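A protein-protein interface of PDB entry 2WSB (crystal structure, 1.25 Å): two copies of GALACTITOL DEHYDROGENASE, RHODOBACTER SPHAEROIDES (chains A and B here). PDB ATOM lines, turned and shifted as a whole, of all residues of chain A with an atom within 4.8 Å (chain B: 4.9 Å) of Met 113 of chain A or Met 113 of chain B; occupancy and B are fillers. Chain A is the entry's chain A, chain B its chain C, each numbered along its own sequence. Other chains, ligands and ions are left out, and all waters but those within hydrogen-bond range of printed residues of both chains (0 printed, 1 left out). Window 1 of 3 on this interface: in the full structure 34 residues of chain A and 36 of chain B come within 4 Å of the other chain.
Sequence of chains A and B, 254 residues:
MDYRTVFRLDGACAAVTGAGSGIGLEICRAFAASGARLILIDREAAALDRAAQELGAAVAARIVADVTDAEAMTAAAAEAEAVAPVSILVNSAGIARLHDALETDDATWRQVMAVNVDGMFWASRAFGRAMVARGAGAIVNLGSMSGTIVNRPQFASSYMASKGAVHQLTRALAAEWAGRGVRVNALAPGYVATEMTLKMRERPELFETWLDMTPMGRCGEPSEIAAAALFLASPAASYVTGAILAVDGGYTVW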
ATOM      1  N   TRP A 109      15.169 -26.566 -26.202  1.00  0.00           N
ATOM      2  CA  TRP A 109      15.415 -25.455 -25.264  1.00  0.00           C
ATOM      3  C   TRP A 109      16.884 -24.998 -25.405  1.00  0.00           C
ATOM      4  O   TRP A 109      17.166 -23.801 -25.541  1.00  0.00           O
ATOM      5  CB  TRP A 109      15.118 -25.990 -23.821  1.00  0.00           C
ATOM      6  CG  TRP A 109      15.451 -24.896 -22.816  1.00  0.00           C
ATOM      7  CD1 TRP A 109      16.656 -24.685 -22.228  1.00  0.00           C
ATOM      8  CD2 TRP A 109      14.575 -23.882 -22.356  1.00  0.00           C
ATOM      9  NE1 TRP A 109      16.619 -23.578 -21.370  1.00  0.00           N
ATOM     10  CE2 TRP A 109      15.349 -23.041 -21.517  1.00  0.00           C
ATOM     11  CE3 TRP A 109      13.194 -23.547 -22.613  1.00  0.00           C
ATOM     12  CZ2 TRP A 109      14.808 -21.913 -20.884  1.00  0.00           C
ATOM     13  CZ3 TRP A 109      12.708 -22.358 -21.962  1.00  0.00           C
ATOM     14  CH2 TRP A 109      13.498 -21.671 -21.053  1.00  0.00           C
ATOM     15  N   ARG A 110      17.815 -25.974 -25.332  1.00  0.00           N
ATOM     16  CA  ARG A 110      19.232 -25.611 -25.332  1.00  0.00           C
ATOM     17  C   ARG A 110      19.622 -24.953 -26.618  1.00  0.00           C
ATOM     18  O   ARG A 110      20.368 -23.957 -26.560  1.00  0.00           O
ATOM     19  CB  ARG A 110      20.083 -26.829 -25.098  1.00  0.00           C
ATOM     20  CG  ARG A 110      20.014 -27.158 -23.572  1.00  0.00           C
ATOM     21  CD  ARG A 110      20.643 -25.872 -22.567  1.00  0.00           C
ATOM     22  NE  ARG A 110      21.680 -25.216 -23.368  1.00  0.00           N
ATOM     23  CZ  ARG A 110      21.748 -23.845 -23.530  1.00  0.00           C
ATOM     24  NH1 ARG A 110      21.056 -23.169 -22.688  1.00  0.00           N
ATOM     25  NH2 ARG A 110      22.693 -23.337 -24.139  1.00  0.00           N
ATOM     26  N   GLN A 111      19.159 -25.446 -27.792  1.00  0.00           N
ATOM     27  CA  GLN A 111      19.464 -24.935 -29.175  1.00  0.00           C
ATOM     28  C   GLN A 111      19.106 -23.404 -29.182  1.00  0.00           C
ATOM     29  O   GLN A 111      19.907 -22.470 -29.466  1.00  0.00           O
ATOM     30  CB  GLN A 111      18.614 -25.713 -30.248  1.00  0.00           C
ATOM     31  CG  GLN A 111      19.071 -25.594 -31.662  1.00  0.00           C
ATOM     32  CD  GLN A 111      18.083 -26.239 -32.710  1.00  0.00           C
ATOM     33  OE1 GLN A 111      17.083 -26.954 -32.381  1.00  0.00           O
ATOM     34  NE2 GLN A 111      18.269 -25.857 -33.941  1.00  0.00           N
ATOM     35  N   VAL A 112      17.843 -23.133 -28.831  1.00  0.00           N
ATOM     36  CA  VAL A 112      17.309 -21.810 -28.999  1.00  0.00           C
ATOM     37  C   VAL A 112      18.049 -20.823 -28.081  1.00  0.00           C
ATOM     38  O   VAL A 112      18.468 -19.706 -28.493  1.00  0.00           O
ATOM     39  CB  VAL A 112      15.775 -21.790 -28.770  1.00  0.00           C
ATOM     40  CG1 VAL A 112      15.250 -20.357 -28.642  1.00  0.00           C
ATOM     41  CG2 VAL A 112      15.063 -22.637 -29.848  1.00  0.00           C
ATOM     42  N   MET A 113      18.304 -21.212 -26.827  1.00  0.00           N
ATOM     43  CA  MET A 113      19.068 -20.326 -25.904  1.00  0.00           C
ATOM     44  C   MET A 113      20.508 -20.156 -26.420  1.00  0.00           C
ATOM     45  O   MET A 113      21.090 -19.047 -26.300  1.00  0.00           O
ATOM     46  CB  MET A 113      19.073 -20.941 -24.521  1.00  0.00           C
ATOM     47  CG  MET A 113      17.652 -20.967 -23.844  1.00  0.00           C
ATOM     48  SD  MET A 113      16.957 -19.272 -23.546  1.00  0.00           S
ATOM     49  CE  MET A 113      17.958 -18.692 -22.285  1.00  0.00           C
ATOM     50  N   ALA A 114      21.126 -21.235 -26.948  1.00  0.00           N
ATOM     51  CA  ALA A 114      22.496 -21.146 -27.395  1.00  0.00           C
ATOM     52  C   ALA A 114      22.673 -20.149 -28.530  1.00  0.00           C
ATOM     53  O   ALA A 114      23.673 -19.361 -28.526  1.00  0.00           O
ATOM     54  CB  ALA A 114      22.984 -22.486 -27.898  1.00  0.00           C
ATOM     55  N   VAL A 115      21.776 -20.193 -29.524  1.00  0.00           N
ATOM     56  CA  VAL A 115      21.949 -19.276 -30.636  1.00  0.00           C
ATOM     57  C   VAL A 115      21.554 -17.858 -30.235  1.00  0.00           C
ATOM     58  O   VAL A 115      22.281 -16.874 -30.445  1.00  0.00           O
ATOM     59  CB  VAL A 115      21.100 -19.683 -31.841  1.00  0.00           C
ATOM     60  CG1 VAL A 115      21.235 -18.607 -33.031  1.00  0.00           C
ATOM     61  CG2 VAL A 115      21.382 -21.105 -32.353  1.00  0.00           C
ATOM     62  N   ASN A 116      20.361 -17.723 -29.608  1.00  0.00           N
ATOM     63  CA  ASN A 116      19.763 -16.409 -29.481  1.00  0.00           C
ATOM     64  C   ASN A 116      20.370 -15.597 -28.355  1.00  0.00           C
ATOM     65  O   ASN A 116      20.335 -14.355 -28.453  1.00  0.00           O
ATOM     66  CB  ASN A 116      18.250 -16.580 -29.174  1.00  0.00           C
ATOM     67  CG  ASN A 116      17.472 -17.045 -30.368  1.00  0.00           C
ATOM     68  OD1 ASN A 116      18.073 -17.369 -31.404  1.00  0.00           O
ATOM     69  ND2 ASN A 116      16.161 -17.124 -30.213  1.00  0.00           N
ATOM     70  N   VAL A 117      20.953 -16.257 -27.311  1.00  0.00           N
ATOM     71  CA  VAL A 117      21.518 -15.576 -26.148  1.00  0.00           C
ATOM     72  C   VAL A 117      23.001 -15.812 -26.098  1.00  0.00           C
ATOM     73  O   VAL A 117      23.806 -14.834 -26.147  1.00  0.00           O
ATOM     74  CB  VAL A 117      20.838 -16.136 -24.793  1.00  0.00           C
ATOM     75  CG1 VAL A 117      21.417 -15.344 -23.593  1.00  0.00           C
ATOM     76  CG2 VAL A 117      19.310 -15.993 -24.930  1.00  0.00           C
ATOM     77  N   ASP A 118      23.404 -17.080 -25.987  1.00  0.00           N
ATOM     78  CA  ASP A 118      24.860 -17.310 -25.785  1.00  0.00           C
ATOM     79  C   ASP A 118      25.627 -16.808 -26.964  1.00  0.00           C
ATOM     80  O   ASP A 118      26.668 -16.126 -26.738  1.00  0.00           O
ATOM     81  CB  ASP A 118      25.183 -18.781 -25.585  1.00  0.00           C
ATOM     82  CG  ASP A 118      24.574 -19.395 -24.317  1.00  0.00           C
ATOM     83  OD1 ASP A 118      23.907 -18.699 -23.501  1.00  0.00           O
ATOM     84  OD2 ASP A 118      24.634 -20.641 -24.210  1.00  0.00           O
ATOM     85  N   SER A 158      10.927 -21.281 -25.111  1.00  0.00           N
ATOM     86  CA  SER A 158      12.364 -21.030 -25.193  1.00  0.00           C
ATOM     87  C   SER A 158      12.647 -19.745 -25.949  1.00  0.00           C
ATOM     88  O   SER A 158      13.601 -19.016 -25.575  1.00  0.00           O
ATOM     89  CB  SER A 158      13.033 -22.200 -25.937  1.00  0.00           C
ATOM     90  OG  SER A 158      12.509 -22.449 -27.198  1.00  0.00           O
ATOM     91  N   ALA A 161      11.870 -16.777 -23.467  1.00  0.00           N
ATOM     92  CA  ALA A 161      12.903 -16.673 -22.494  1.00  0.00           C
ATOM     93  C   ALA A 161      14.178 -16.119 -23.149  1.00  0.00           C
ATOM     94  O   ALA A 161      14.841 -15.239 -22.572  1.00  0.00           O
ATOM     95  CB  ALA A 161      13.192 -18.034 -21.875  1.00  0.00           C
ATOM     96  N   SER A 162      14.498 -16.594 -24.386  1.00  0.00           N
ATOM     97  CA  SER A 162      15.746 -16.118 -24.975  1.00  0.00           C
ATOM     98  C   SER A 162      15.656 -14.629 -25.248  1.00  0.00           C
ATOM     99  O   SER A 162      16.696 -13.924 -25.141  1.00  0.00           O
ATOM    100  CB  SER A 162      16.015 -16.896 -26.280  1.00  0.00           C
ATOM    101  OG  SER A 162      15.246 -16.452 -27.422  1.00  0.00           O
ATOM    102  N   ALA A 165      16.220 -12.555 -22.254  1.00  0.00           N
ATOM    103  CA  ALA A 165      17.639 -12.507 -21.965  1.00  0.00           C
ATOM    104  C   ALA A 165      18.309 -11.544 -22.944  1.00  0.00           C
ATOM    105  O   ALA A 165      19.222 -10.816 -22.513  1.00  0.00           O
ATOM    106  CB  ALA A 165      18.297 -13.878 -22.126  1.00  0.00           C
ATOM    107  N   TRP B 109      29.636 -17.909 -17.951  1.00  0.00           N
ATOM    108  CA  TRP B 109      28.352 -17.547 -18.567  1.00  0.00           C
ATOM    109  C   TRP B 109      27.362 -18.748 -18.641  1.00  0.00           C
ATOM    110  O   TRP B 109      26.222 -18.641 -18.207  1.00  0.00           O
ATOM    111  CB  TRP B 109      28.663 -17.079 -20.011  1.00  0.00           C
ATOM    112  CG  TRP B 109      27.444 -16.738 -20.785  1.00  0.00           C
ATOM    113  CD1 TRP B 109      26.616 -17.606 -21.512  1.00  0.00           C
ATOM    114  CD2 TRP B 109      26.795 -15.434 -20.809  1.00  0.00           C
ATOM    115  NE1 TRP B 109      25.518 -16.887 -21.953  1.00  0.00           N
ATOM    116  CE2 TRP B 109      25.617 -15.571 -21.554  1.00  0.00           C
ATOM    117  CE3 TRP B 109      27.153 -14.165 -20.236  1.00  0.00           C
ATOM    118  CZ2 TRP B 109      24.743 -14.425 -21.780  1.00  0.00           C
ATOM    119  CZ3 TRP B 109      26.335 -13.061 -20.475  1.00  0.00           C
ATOM    120  CH2 TRP B 109      25.204 -13.246 -21.176  1.00  0.00           C
ATOM    121  N   ARG B 110      27.900 -19.904 -19.035  1.00  0.00           N
ATOM    122  CA  ARG B 110      27.042 -21.082 -19.298  1.00  0.00           C
ATOM    123  C   ARG B 110      26.381 -21.561 -18.014  1.00  0.00           C
ATOM    124  O   ARG B 110      25.219 -21.957 -18.006  1.00  0.00           O
ATOM    125  CB  ARG B 110      27.954 -22.197 -19.774  1.00  0.00           C
ATOM    126  CG  ARG B 110      28.110 -22.088 -21.260  1.00  0.00           C
ATOM    127  CD  ARG B 110      26.722 -21.997 -21.898  1.00  0.00           C
ATOM    128  NE  ARG B 110      25.729 -22.947 -21.295  1.00  0.00           N
ATOM    129  CZ  ARG B 110      24.398 -22.687 -21.062  1.00  0.00           C
ATOM    130  NH1 ARG B 110      23.862 -21.596 -21.566  1.00  0.00           N
ATOM    131  NH2 ARG B 110      23.676 -23.575 -20.549  1.00  0.00           N
ATOM    132  N   GLN B 111      27.110 -21.529 -16.925  1.00  0.00           N
ATOM    133  CA  GLN B 111      26.604 -22.159 -15.762  1.00  0.00           C
ATOM    134  C   GLN B 111      25.666 -21.203 -15.054  1.00  0.00           C
ATOM    135  O   GLN B 111      24.640 -21.668 -14.549  1.00  0.00           O
ATOM    136  CB  GLN B 111      27.732 -22.528 -14.868  1.00  0.00           C
ATOM    137  CG  GLN B 111      27.332 -23.130 -13.452  1.00  0.00           C
ATOM    138  CD  GLN B 111      26.666 -24.506 -13.431  1.00  0.00           C
ATOM    139  OE1 GLN B 111      26.372 -25.016 -12.324  1.00  0.00           O
ATOM    140  NE2 GLN B 111      26.675 -25.203 -14.567  1.00  0.00           N
ATOM    141  N   VAL B 112      25.924 -19.865 -15.049  1.00  0.00           N
ATOM    142  CA  VAL B 112      24.880 -18.992 -14.521  1.00  0.00           C
ATOM    143  C   VAL B 112      23.570 -19.174 -15.241  1.00  0.00           C
ATOM    144  O   VAL B 112      22.499 -19.274 -14.644  1.00  0.00           O
ATOM    145  CB  VAL B 112      25.400 -17.514 -14.551  1.00  0.00           C
ATOM    146  CG1 VAL B 112      24.238 -16.563 -14.171  1.00  0.00           C
ATOM    147  CG2 VAL B 112      26.574 -17.376 -13.583  1.00  0.00           C
ATOM    148  N   MET B 113      23.587 -19.264 -16.585  1.00  0.00           N
ATOM    149  CA  MET B 113      22.372 -19.479 -17.337  1.00  0.00           C
ATOM    150  C   MET B 113      21.828 -20.890 -17.022  1.00  0.00           C
ATOM    151  O   MET B 113      20.598 -21.059 -17.015  1.00  0.00           O
ATOM    152  CB  MET B 113      22.608 -19.268 -18.864  1.00  0.00           C
ATOM    153  CG  MET B 113      23.153 -17.848 -19.139  1.00  0.00           C
ATOM    154  SD  MET B 113      21.866 -16.546 -19.111  1.00  0.00           S
ATOM    155  CE  MET B 113      20.614 -17.116 -20.449  1.00  0.00           C
ATOM    156  N   ALA B 114      22.694 -21.876 -16.856  1.00  0.00           N
ATOM    157  CA  ALA B 114      22.208 -23.241 -16.653  1.00  0.00           C
ATOM    158  C   ALA B 114      21.406 -23.320 -15.322  1.00  0.00           C
ATOM    159  O   ALA B 114      20.349 -23.982 -15.279  1.00  0.00           O
ATOM    160  CB  ALA B 114      23.393 -24.198 -16.587  1.00  0.00           C
ATOM    161  N   VAL B 115      21.908 -22.704 -14.247  1.00  0.00           N
ATOM    162  CA  VAL B 115      21.194 -22.800 -12.955  1.00  0.00           C
ATOM    163  C   VAL B 115      19.936 -21.888 -13.077  1.00  0.00           C
ATOM    164  O   VAL B 115      18.830 -22.319 -12.734  1.00  0.00           O
ATOM    165  CB  VAL B 115      22.043 -22.380 -11.704  1.00  0.00           C
ATOM    166  CG1 VAL B 115      21.170 -22.528 -10.498  1.00  0.00           C
ATOM    167  CG2 VAL B 115      23.312 -23.250 -11.733  1.00  0.00           C
ATOM    168  N   ASN B 116      20.149 -20.634 -13.437  1.00  0.00           N
ATOM    169  CA  ASN B 116      19.124 -19.643 -13.220  1.00  0.00           C
ATOM    170  C   ASN B 116      17.972 -19.722 -14.176  1.00  0.00           C
ATOM    171  O   ASN B 116      16.882 -19.302 -13.790  1.00  0.00           O
ATOM    172  CB  ASN B 116      19.761 -18.241 -13.318  1.00  0.00           C
ATOM    173  CG  ASN B 116      20.683 -17.930 -12.131  1.00  0.00           C
ATOM    174  OD1 ASN B 116      20.891 -18.788 -11.241  1.00  0.00           O
ATOM    175  ND2 ASN B 116      21.183 -16.688 -12.064  1.00  0.00           N
ATOM    176  N   VAL B 117      18.240 -20.186 -15.418  1.00  0.00           N
ATOM    177  CA  VAL B 117      17.244 -20.236 -16.476  1.00  0.00           C
ATOM    178  C   VAL B 117      16.934 -21.693 -16.763  1.00  0.00           C
ATOM    179  O   VAL B 117      15.755 -22.138 -16.570  1.00  0.00           O
ATOM    180  CB  VAL B 117      17.734 -19.561 -17.780  1.00  0.00           C
ATOM    181  CG1 VAL B 117      16.655 -19.608 -18.806  1.00  0.00           C
ATOM    182  CG2 VAL B 117      18.182 -18.132 -17.422  1.00  0.00           C
ATOM    183  N   ASP B 118      17.923 -22.422 -17.298  1.00  0.00           N
ATOM    184  CA  ASP B 118      17.637 -23.815 -17.740  1.00  0.00           C
ATOM    185  C   ASP B 118      17.079 -24.624 -16.598  1.00  0.00           C
ATOM    186  O   ASP B 118      16.067 -25.330 -16.880  1.00  0.00           O
ATOM    187  CB  ASP B 118      18.857 -24.534 -18.282  1.00  0.00           C
ATOM    188  CG  ASP B 118      19.537 -23.811 -19.431  1.00  0.00           C
ATOM    189  OD1 ASP B 118      18.962 -22.850 -20.023  1.00  0.00           O
ATOM    190  OD2 ASP B 118      20.731 -24.247 -19.725  1.00  0.00           O
ATOM    191  N   GLY B 119      17.670 -24.536 -15.410  1.00  0.00           N
ATOM    192  CA  GLY B 119      17.153 -25.367 -14.302  1.00  0.00           C
ATOM    193  C   GLY B 119      15.762 -24.972 -13.913  1.00  0.00           C
ATOM    194  O   GLY B 119      14.939 -25.853 -13.533  1.00  0.00           O
ATOM    195  N   SER B 158      25.931 -12.058 -17.146  1.00  0.00           N
ATOM    196  CA  SER B 158      25.208 -13.360 -17.245  1.00  0.00           C
ATOM    197  C   SER B 158      24.031 -13.322 -16.263  1.00  0.00           C
ATOM    198  O   SER B 158      22.970 -13.942 -16.518  1.00  0.00           O
ATOM    199  CB  SER B 158      26.128 -14.539 -16.926  1.00  0.00           C
ATOM    200  OG  SER B 158      26.739 -14.414 -15.618  1.00  0.00           O
ATOM    201  N   ALA B 161      21.236 -11.174 -17.821  1.00  0.00           N
ATOM    202  CA  ALA B 161      20.577 -11.860 -18.929  1.00  0.00           C
ATOM    203  C   ALA B 161      19.779 -13.023 -18.398  1.00  0.00           C
ATOM    204  O   ALA B 161      18.653 -13.235 -18.867  1.00  0.00           O
ATOM    205  CB  ALA B 161      21.714 -12.368 -19.881  1.00  0.00           C
ATOM    206  N   SER B 162      20.250 -13.749 -17.384  1.00  0.00           N
ATOM    207  CA  SER B 162      19.522 -14.906 -16.860  1.00  0.00           C
ATOM    208  C   SER B 162      18.175 -14.433 -16.261  1.00  0.00           C
ATOM    209  O   SER B 162      17.174 -15.146 -16.382  1.00  0.00           O
ATOM    210  CB  SER B 162      20.323 -15.738 -15.886  1.00  0.00           C
ATOM    211  OG  SER B 162      20.408 -15.113 -14.590  1.00  0.00           O
ATOM    212  N   ALA B 165      15.629 -13.623 -18.786  1.00  0.00           N
ATOM    213  CA  ALA B 165      15.015 -14.887 -19.264  1.00  0.00           C
ATOM    214  C   ALA B 165      14.062 -15.389 -18.246  1.00  0.00           C
ATOM    215  O   ALA B 165      12.991 -15.889 -18.619  1.00  0.00           O
ATOM    216  CB  ALA B 165      16.131 -15.879 -19.537  1.00  0.00           C
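OD2 of Asp 118 of chain B lies within salt-bridge range of NH1 of Arg 110 of chain A (3.2 Å). The guanidinium group of Arg 110 of chain B sits close to the guanidinium group of Arg 110 of chain A, 3.3 Å away. The side-chain carboxylate of Asp 118 of chain A lies within hydrogen-bond range of the indole nitrogen of Trp 109 of chain B, at 2.9 Å. The guanidinium group (NH1) of Arg 110 of chain B is in salt-bridge range of the side-chain carboxylate (OD2) of Asp 118 of chain A. OD1 of Asp 118 of chain B lies within hydrogen-bond range of NE1 of Trp 109 of chain A (2.8 Å).
The side-chain carboxylate (OD2) of Asp 118 of chain A lies within salt-bridge range of the guanidinium group (NH2) of Arg 110 of chain A (3.3 Å). The side-chain sulfur (SD) of Met 113 of chain B sits close to the backbone NH (N) of Ser 162 of chain B (3.7 Å). The backbone carbonyl oxygen (O) of Met 113 of chain A is in hydrogen-bond range of the backbone NH (N) of Asp 118 of chain A (3.1 Å). O of Met 113 of chain B is in hydrogen-bond range of N of Asp 118 of chain B (3.0 Å). SD of Met 113 of chain A lies close to N of Ser 162 of chain A (3.7 Å). NH2 of Arg 110 of chain B lies within salt-bridge range of OD2 of Asp 118 of chain B, 3.1 Å away.
CZ2 of Trp 109 of chain A touches CG1 of Val 117 of chain B, 3.6 Å away. CE of Met 113 of chain A touches CE of Met 113 of chain B, at 3.6 Å. Met 113 of chain A touches Val 117 of chain B. CG1 of Val 117 of chain A touches CZ2 of Trp 109 of chain B, at 3.9 Å. Met 113 of chain B touches Val 117 of chain A. O of Ala 161 of chain A touches CA of Ala 165 of chain B (3.3 Å). Ala 161 of chain B touches Ala 165 of chain A (O to CA, 3.3 Å). Ala 165 of chain A touches Ala 165 of chain B (N to N, 3.7 Å).
Of the printed residues of chain B, Met 113 of chain A touches Met 113 and Val 117. Asn 116 of chain A touches none of the printed residues of chain B. Of the printed residues of chain B, Asp 118 of chain A touches Trp 109 and Arg 110. Of the printed residues of chain A, Trp 109 of chain B touches Val 117 and Asp 118. Printed residues of chain A within 4 Å of Arg 110 of chain B: Arg 110 (3.3 Å) and Asp 118 (2.9 Å). Gln 111 of chain B touches none of the printed residues of chain A. Of the printed residues of chain A, Val 117 of chain B touches Trp 109 (3.6 Å) and Met 113 (3.8 Å).
Of the 14 printed residues of chain A, 7 touch a printed residue of chain B. Among the printed residues, Asp or Glu carboxylates within 4 Å of a Lys or Arg side-chain nitrogen of the other chain: Arg 110 of chain A with Asp 118 of chain B and Asp 118 of chain A with Arg 110 of chain B.
Trp 109 of chain A touches Val 117 of chain B, and with the chains exchanged Val 117 of chain A touches Trp 109 of chain B. Arg 110 of chain A touches Asp 118 of chain B, and with the chains exchanged Asp 118 of chain A touches Arg 110 of chain B. Met 113 of chain A touches Val 117 of chain B, and with the chains exchanged Val 117 of chain A touches Met 113 of chain B. Ala 161 of chain A touches Ala 165 of chain B, and with the chains exchanged Ala 165 of chain A touches Ala 161 of chain B. 14 positions are printed for both chains.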
